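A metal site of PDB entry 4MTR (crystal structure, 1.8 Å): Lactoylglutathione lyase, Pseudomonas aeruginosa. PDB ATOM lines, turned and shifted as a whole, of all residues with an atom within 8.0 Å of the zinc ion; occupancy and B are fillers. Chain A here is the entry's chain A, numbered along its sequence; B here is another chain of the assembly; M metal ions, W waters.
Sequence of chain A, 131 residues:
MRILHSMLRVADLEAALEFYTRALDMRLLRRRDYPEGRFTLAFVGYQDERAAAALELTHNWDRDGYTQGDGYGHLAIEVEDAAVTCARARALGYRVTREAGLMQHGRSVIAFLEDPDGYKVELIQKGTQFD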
ATOM      1  N   LEU A   4      -8.567  24.853  18.622  1.00  0.00           N
ATOM      2  CA  LEU A   4      -7.730  24.565  17.467  1.00  0.00           C
ATOM      3  C   LEU A   4      -8.023  23.221  16.873  1.00  0.00           C
ATOM      4  O   LEU A   4      -8.142  23.109  15.657  1.00  0.00           O
ATOM      5  CB  LEU A   4      -6.245  24.601  17.837  1.00  0.00           C
ATOM      6  CG  LEU A   4      -5.715  25.965  18.226  1.00  0.00           C
ATOM      7  CD1 LEU A   4      -4.277  25.853  18.719  1.00  0.00           C
ATOM      8  CD2 LEU A   4      -5.826  26.965  17.069  1.00  0.00           C
ATOM      9  N   HIS A   5      -8.074  22.174  17.734  1.00  0.00           N
ATOM     10  CA  HIS A   5      -8.304  20.803  17.262  1.00  0.00           C
ATOM     11  C   HIS A   5      -8.529  19.829  18.416  1.00  0.00           C
ATOM     12  O   HIS A   5      -8.192  20.132  19.549  1.00  0.00           O
ATOM     13  CB  HIS A   5      -7.093  20.315  16.380  1.00  0.00           C
ATOM     14  CG  HIS A   5      -5.761  20.244  17.083  1.00  0.00           C
ATOM     15  ND1 HIS A   5      -4.825  21.276  16.982  1.00  0.00           N
ATOM     16  CD2 HIS A   5      -5.270  19.295  17.919  1.00  0.00           C
ATOM     17  CE1 HIS A   5      -3.769  20.892  17.719  1.00  0.00           C
ATOM     18  NE2 HIS A   5      -3.990  19.708  18.297  1.00  0.00           N
ATOM     19  N   SER A   6      -9.089  18.635  18.099  1.00  0.00           N
ATOM     20  CA  SER A   6      -9.200  17.478  18.963  1.00  0.00           C
ATOM     21  C   SER A   6      -8.139  16.543  18.410  1.00  0.00           C
ATOM     22  O   SER A   6      -7.892  16.587  17.209  1.00  0.00           O
ATOM     23  CB  SER A   6     -10.576  16.836  18.778  1.00  0.00           C
ATOM     24  OG  SER A   6     -10.657  15.596  19.455  1.00  0.00           O
ATOM     25  N   MET A   7      -7.569  15.664  19.241  1.00  0.00           N
ATOM     26  CA  MET A   7      -6.607  14.689  18.756  1.00  0.00           C
ATOM     27  C   MET A   7      -7.090  13.268  19.101  1.00  0.00           C
ATOM     28  O   MET A   7      -7.511  13.021  20.224  1.00  0.00           O
ATOM     29  CB  MET A   7      -5.184  14.938  19.306  1.00  0.00           C
ATOM     30  CG  MET A   7      -4.122  13.992  18.702  1.00  0.00           C
ATOM     31  SD  MET A   7      -4.061  12.304  19.414  1.00  0.00           S
ATOM     32  CE  MET A   7      -2.765  12.513  20.686  1.00  0.00           C
ATOM     33  N   LEU A   8      -7.061  12.382  18.107  1.00  0.00           N
ATOM     34  CA  LEU A   8      -7.462  10.958  18.224  1.00  0.00           C
ATOM     35  C   LEU A   8      -6.339  10.085  17.740  1.00  0.00           C
ATOM     36  O   LEU A   8      -5.693  10.408  16.749  1.00  0.00           O
ATOM     37  CB  LEU A   8      -8.706  10.697  17.360  1.00  0.00           C
ATOM     38  CG  LEU A   8      -9.995  11.515  17.701  1.00  0.00           C
ATOM     39  CD1 LEU A   8     -11.133  11.213  16.686  1.00  0.00           C
ATOM     40  CD2 LEU A   8     -10.474  11.242  19.129  1.00  0.00           C
ATOM     41  N   ARG A  30      -1.635  19.219   7.267  1.00  0.00           N
ATOM     42  CA  ARG A  30      -0.201  18.962   7.438  1.00  0.00           C
ATOM     43  C   ARG A  30       0.017  17.583   7.964  1.00  0.00           C
ATOM     44  O   ARG A  30      -0.902  17.000   8.541  1.00  0.00           O
ATOM     45  CB  ARG A  30       0.581  20.045   8.205  1.00  0.00           C
ATOM     46  CG  ARG A  30       0.331  20.116   9.689  1.00  0.00           C
ATOM     47  CD  ARG A  30       0.870  21.423  10.241  1.00  0.00           C
ATOM     48  NE  ARG A  30      -0.022  21.858  11.322  1.00  0.00           N
ATOM     49  CZ  ARG A  30       0.225  21.683  12.612  1.00  0.00           C
ATOM     50  NH1 ARG A  30       1.366  21.155  13.012  1.00  0.00           N
ATOM     51  NH2 ARG A  30      -0.658  22.086  13.510  1.00  0.00           N
ATOM     52  N   LEU A  41       1.904  12.317  12.811  1.00  0.00           N
ATOM     53  CA  LEU A  41       0.743  13.145  13.018  1.00  0.00           C
ATOM     54  C   LEU A  41       0.216  13.535  11.650  1.00  0.00           C
ATOM     55  O   LEU A  41       1.008  13.821  10.735  1.00  0.00           O
ATOM     56  CB  LEU A  41       1.123  14.482  13.708  1.00  0.00           C
ATOM     57  CG  LEU A  41       1.852  14.473  15.033  1.00  0.00           C
ATOM     58  CD1 LEU A  41       1.988  15.894  15.551  1.00  0.00           C
ATOM     59  CD2 LEU A  41       1.070  13.680  16.088  1.00  0.00           C
ATOM     60  N   PHE A  43      -2.905  16.362  10.344  1.00  0.00           N
ATOM     61  CA  PHE A  43      -3.975  17.273  10.665  1.00  0.00           C
ATOM     62  C   PHE A  43      -4.860  17.300   9.438  1.00  0.00           C
ATOM     63  O   PHE A  43      -4.358  17.489   8.312  1.00  0.00           O
ATOM     64  CB  PHE A  43      -3.458  18.685  10.985  1.00  0.00           C
ATOM     65  CG  PHE A  43      -2.719  18.757  12.317  1.00  0.00           C
ATOM     66  CD1 PHE A  43      -1.414  18.287  12.434  1.00  0.00           C
ATOM     67  CD2 PHE A  43      -3.339  19.278  13.451  1.00  0.00           C
ATOM     68  CE1 PHE A  43      -0.723  18.357  13.662  1.00  0.00           C
ATOM     69  CE2 PHE A  43      -2.650  19.347  14.670  1.00  0.00           C
ATOM     70  CZ  PHE A  43      -1.357  18.866  14.778  1.00  0.00           C
ATOM     71  N   GLU A  49      -5.722  25.870   9.387  1.00  0.00           N
ATOM     72  CA  GLU A  49      -5.739  25.864  10.862  1.00  0.00           C
ATOM     73  C   GLU A  49      -5.837  27.253  11.492  1.00  0.00           C
ATOM     74  O   GLU A  49      -6.377  27.394  12.599  1.00  0.00           O
ATOM     75  CB  GLU A  49      -4.531  25.109  11.397  1.00  0.00           C
ATOM     76  CG  GLU A  49      -4.605  23.623  11.113  1.00  0.00           C
ATOM     77  CD  GLU A  49      -3.353  22.907  11.558  1.00  0.00           C
ATOM     78  OE1 GLU A  49      -3.252  22.568  12.755  1.00  0.00           O
ATOM     79  OE2 GLU A  49      -2.465  22.715  10.696  1.00  0.00           O
ATOM     80  N   LEU A  55      -8.818  18.434  12.949  1.00  0.00           N
ATOM     81  CA  LEU A  55      -8.790  17.145  13.608  1.00  0.00           C
ATOM     82  C   LEU A  55      -7.365  16.613  13.482  1.00  0.00           C
ATOM     83  O   LEU A  55      -6.848  16.521  12.368  1.00  0.00           O
ATOM     84  CB  LEU A  55      -9.813  16.171  12.982  1.00  0.00           C
ATOM     85  CG  LEU A  55      -9.756  14.720  13.507  1.00  0.00           C
ATOM     86  CD1 LEU A  55     -10.097  14.650  15.040  1.00  0.00           C
ATOM     87  CD2 LEU A  55     -10.643  13.794  12.674  1.00  0.00           C
ATOM     88  N   GLU A  56      -6.728  16.310  14.615  1.00  0.00           N
ATOM     89  CA  GLU A  56      -5.385  15.768  14.594  1.00  0.00           C
ATOM     90  C   GLU A  56      -5.437  14.269  14.733  1.00  0.00           C
ATOM     91  O   GLU A  56      -6.052  13.726  15.652  1.00  0.00           O
ATOM     92  CB  GLU A  56      -4.561  16.378  15.749  1.00  0.00           C
ATOM     93  CG  GLU A  56      -3.115  15.879  15.801  1.00  0.00           C
ATOM     94  CD  GLU A  56      -2.342  16.409  17.006  1.00  0.00           C
ATOM     95  OE1 GLU A  56      -2.966  17.035  17.895  1.00  0.00           O
ATOM     96  OE2 GLU A  56      -1.097  16.256  17.036  1.00  0.00           O
ATOM     97  N   LEU A  57      -4.756  13.584  13.876  1.00  0.00           N
ATOM     98  CA  LEU A  57      -4.700  12.125  13.934  1.00  0.00           C
ATOM     99  C   LEU A  57      -3.297  11.690  14.267  1.00  0.00           C
ATOM    100  O   LEU A  57      -2.364  12.122  13.588  1.00  0.00           O
ATOM    101  CB  LEU A  57      -5.056  11.578  12.555  1.00  0.00           C
ATOM    102  CG  LEU A  57      -6.482  11.901  12.086  1.00  0.00           C
ATOM    103  CD1 LEU A  57      -6.680  11.425  10.688  1.00  0.00           C
ATOM    104  CD2 LEU A  57      -7.558  11.271  13.037  1.00  0.00           C
ATOM    105  N   THR A  58      -3.145  10.818  15.262  1.00  0.00           N
ATOM    106  CA  THR A  58      -1.830  10.323  15.671  1.00  0.00           C
ATOM    107  C   THR A  58      -1.730   8.811  15.510  1.00  0.00           C
ATOM    108  O   THR A  58      -2.610   8.106  15.950  1.00  0.00           O
ATOM    109  CB  THR A  58      -1.571  10.671  17.173  1.00  0.00           C
ATOM    110  OG1 THR A  58      -1.599  12.094  17.334  1.00  0.00           O
ATOM    111  CG2 THR A  58      -0.238  10.137  17.682  1.00  0.00           C
ATOM    112  N   GLY B  73      -7.024  11.635  22.521  1.00  0.00           N
ATOM    113  CA  GLY B  73      -5.788  12.317  22.841  1.00  0.00           C
ATOM    114  C   GLY B  73      -6.005  13.528  23.709  1.00  0.00           C
ATOM    115  O   GLY B  73      -5.706  13.482  24.896  1.00  0.00           O
ATOM    116  N   HIS B  74      -6.418  14.653  23.100  1.00  0.00           N
ATOM    117  CA  HIS B  74      -6.565  15.933  23.792  1.00  0.00           C
ATOM    118  C   HIS B  74      -7.368  16.908  22.969  1.00  0.00           C
ATOM    119  O   HIS B  74      -7.717  16.625  21.827  1.00  0.00           O
ATOM    120  CB  HIS B  74      -5.180  16.537  24.087  1.00  0.00           C
ATOM    121  CG  HIS B  74      -4.328  16.728  22.869  1.00  0.00           C
ATOM    122  ND1 HIS B  74      -3.294  15.867  22.573  1.00  0.00           N
ATOM    123  CD2 HIS B  74      -4.385  17.682  21.907  1.00  0.00           C
ATOM    124  CE1 HIS B  74      -2.757  16.316  21.436  1.00  0.00           C
ATOM    125  NE2 HIS B  74      -3.383  17.391  20.997  1.00  0.00           N
ATOM    126  N   LEU B  75      -7.652  18.065  23.565  1.00  0.00           N
ATOM    127  CA  LEU B  75      -8.289  19.216  22.954  1.00  0.00           C
ATOM    128  C   LEU B  75      -7.237  20.332  23.004  1.00  0.00           C
ATOM    129  O   LEU B  75      -6.686  20.597  24.080  1.00  0.00           O
ATOM    130  CB  LEU B  75      -9.527  19.652  23.740  1.00  0.00           C
ATOM    131  CG  LEU B  75     -10.334  20.811  23.087  1.00  0.00           C
ATOM    132  CD1 LEU B  75     -10.974  20.350  21.776  1.00  0.00           C
ATOM    133  CD2 LEU B  75     -11.411  21.342  24.047  1.00  0.00           C
ATOM    134  N   ALA B  76      -6.935  20.927  21.864  1.00  0.00           N
ATOM    135  CA  ALA B  76      -5.967  22.029  21.776  1.00  0.00           C
ATOM    136  C   ALA B  76      -6.717  23.318  21.689  1.00  0.00           C
ATOM    137  O   ALA B  76      -7.769  23.412  21.018  1.00  0.00           O
ATOM    138  CB  ALA B  76      -5.069  21.862  20.567  1.00  0.00           C
ATOM    139  N   ILE B  77      -6.229  24.307  22.449  1.00  0.00           N
ATOM    140  CA  ILE B  77      -6.796  25.641  22.543  1.00  0.00           C
ATOM    141  C   ILE B  77      -5.725  26.652  22.286  1.00  0.00           C
ATOM    142  O   ILE B  77      -4.622  26.546  22.837  1.00  0.00           O
ATOM    143  CB  ILE B  77      -7.527  25.884  23.894  1.00  0.00           C
ATOM    144  CG1 ILE B  77      -8.769  24.968  23.995  1.00  0.00           C
ATOM    145  CG2 ILE B  77      -7.975  27.380  24.035  1.00  0.00           C
ATOM    146  CD1 ILE B  77      -9.263  24.812  25.282  1.00  0.00           C
ATOM    147  N   ILE B 110       4.088  25.575  24.059  1.00  0.00           N
ATOM    148  CA  ILE B 110       3.011  24.604  24.285  1.00  0.00           C
ATOM    149  C   ILE B 110       3.036  24.058  25.733  1.00  0.00           C
ATOM    150  O   ILE B 110       4.119  23.811  26.280  1.00  0.00           O
ATOM    151  CB  ILE B 110       3.058  23.456  23.202  1.00  0.00           C
ATOM    152  CG1 ILE B 110       2.862  24.010  21.764  1.00  0.00           C
ATOM    153  CG2 ILE B 110       2.019  22.376  23.464  1.00  0.00           C
ATOM    154  N   PHE B 112       0.318  21.499  28.732  1.00  0.00           N
ATOM    155  CA  PHE B 112      -0.773  20.557  28.939  1.00  0.00           C
ATOM    156  C   PHE B 112      -1.405  20.652  30.327  1.00  0.00           C
ATOM    157  O   PHE B 112      -0.700  20.528  31.333  1.00  0.00           O
ATOM    158  CB  PHE B 112      -0.255  19.131  28.734  1.00  0.00           C
ATOM    159  CG  PHE B 112      -0.374  18.606  27.323  1.00  0.00           C
ATOM    160  CD1 PHE B 112      -1.540  18.003  26.887  1.00  0.00           C
ATOM    161  CD2 PHE B 112       0.700  18.716  26.443  1.00  0.00           C
ATOM    162  CE1 PHE B 112      -1.642  17.510  25.574  1.00  0.00           C
ATOM    163  CE2 PHE B 112       0.600  18.223  25.140  1.00  0.00           C
ATOM    164  CZ  PHE B 112      -0.564  17.610  24.715  1.00  0.00           C
ATOM    165  N   VAL B 121      -5.776  18.964  28.034  1.00  0.00           N
ATOM    166  CA  VAL B 121      -5.979  20.179  27.295  1.00  0.00           C
ATOM    167  C   VAL B 121      -4.617  20.711  26.875  1.00  0.00           C
ATOM    168  O   VAL B 121      -3.760  20.947  27.726  1.00  0.00           O
ATOM    169  CB  VAL B 121      -6.836  21.230  28.034  1.00  0.00           C
ATOM    170  CG1 VAL B 121      -6.970  22.484  27.170  1.00  0.00           C
ATOM    171  CG2 VAL B 121      -8.224  20.676  28.367  1.00  0.00           C
ATOM    172  N   GLU B 122      -4.399  20.813  25.566  1.00  0.00           N
ATOM    173  CA  GLU B 122      -3.126  21.331  25.040  1.00  0.00           C
ATOM    174  C   GLU B 122      -3.252  22.846  24.820  1.00  0.00           C
ATOM    175  O   GLU B 122      -4.161  23.263  24.118  1.00  0.00           O
ATOM    176  CB  GLU B 122      -2.832  20.613  23.713  1.00  0.00           C
ATOM    177  CG  GLU B 122      -1.495  20.961  23.078  1.00  0.00           C
ATOM    178  CD  GLU B 122      -1.247  20.322  21.727  1.00  0.00           C
ATOM    179  OE1 GLU B 122      -2.200  20.206  20.910  1.00  0.00           O
ATOM    180  OE2 GLU B 122      -0.068  20.073  21.425  1.00  0.00           O
ATOM    181  N   LEU B 123      -2.352  23.669  25.430  1.00  0.00           N
ATOM    182  CA  LEU B 123      -2.393  25.125  25.227  1.00  0.00           C
ATOM    183  C   LEU B 123      -1.346  25.493  24.215  1.00  0.00           C
ATOM    184  O   LEU B 123      -0.204  25.101  24.389  1.00  0.00           O
ATOM    185  CB  LEU B 123      -2.133  25.911  26.537  1.00  0.00           C
ATOM    186  CG  LEU B 123      -3.028  25.528  27.726  1.00  0.00           C
ATOM    187  CD1 LEU B 123      -2.565  26.265  28.972  1.00  0.00           C
ATOM    188  CD2 LEU B 123      -4.497  25.793  27.408  1.00  0.00           C
ATOM    189  N   ILE B 124      -1.723  26.190  23.141  1.00  0.00           N
ATOM    190  CA  ILE B 124      -0.763  26.556  22.094  1.00  0.00           C
ATOM    191  C   ILE B 124      -0.782  28.065  22.018  1.00  0.00           C
ATOM    192  O   ILE B 124      -1.836  28.657  21.774  1.00  0.00           O
ATOM    193  CB  ILE B 124      -1.075  25.880  20.729  1.00  0.00           C
ATOM    194  CG1 ILE B 124      -1.196  24.340  20.871  1.00  0.00           C
ATOM    195  CG2 ILE B 124      -0.031  26.286  19.636  1.00  0.00           C
ATOM    196  CD1 ILE B 124      -1.471  23.555  19.593  1.00  0.00           C
HETATM  197 ZN    ZN M   1      -2.691  18.605  19.452  1.00  0.00          ZN
HETATM  198  O   HOH W   1      -0.833  18.413  19.031  1.00  0.00           O
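N of Leu 8 lies within hydrogen-bond range of O of Glu 56 (3.0 Å).
The backbone NH of Glu 56 is in hydrogen-bond range of the backbone carbonyl oxygen of Ser 6, 2.9 Å away.
O of Glu 122 of chain B is in hydrogen-bond range of N of Ile 77 of chain B (2.9 Å).
N of Glu 122 of chain B is in hydrogen-bond range of O of Leu 75 of chain B.
The backbone NH (N) of Ala 76 of chain B is in hydrogen-bond range of the backbone carbonyl oxygen (O) of His 5, 2.8 Å away.
O of His 74 of chain B is in hydrogen-bond range of N of Met 7 (2.8 Å).
Four residues have an atom within 4 Å of the zinc ion: His 5, Glu 56, His 74 of chain B and Glu 122 of chain B.
The zinc ion is bound by water W1 (1.9 Å).
NE2 of His 5 binds the zinc ion (2.1 Å).
The zinc ion is bound by NE2 of His 74 of chain B, at 2.1 Å.
OE1 of Glu 122 of chain B binds the zinc ion.
The zinc ion is bound by the side-chain carboxylate (OE1) of Glu 56.
Water W1 bridges the side-chain carboxylate (OE2) of Glu 56 (2.9 Å) and the side-chain carboxylate (OE2) of Glu 122 of chain B (3.0 Å).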
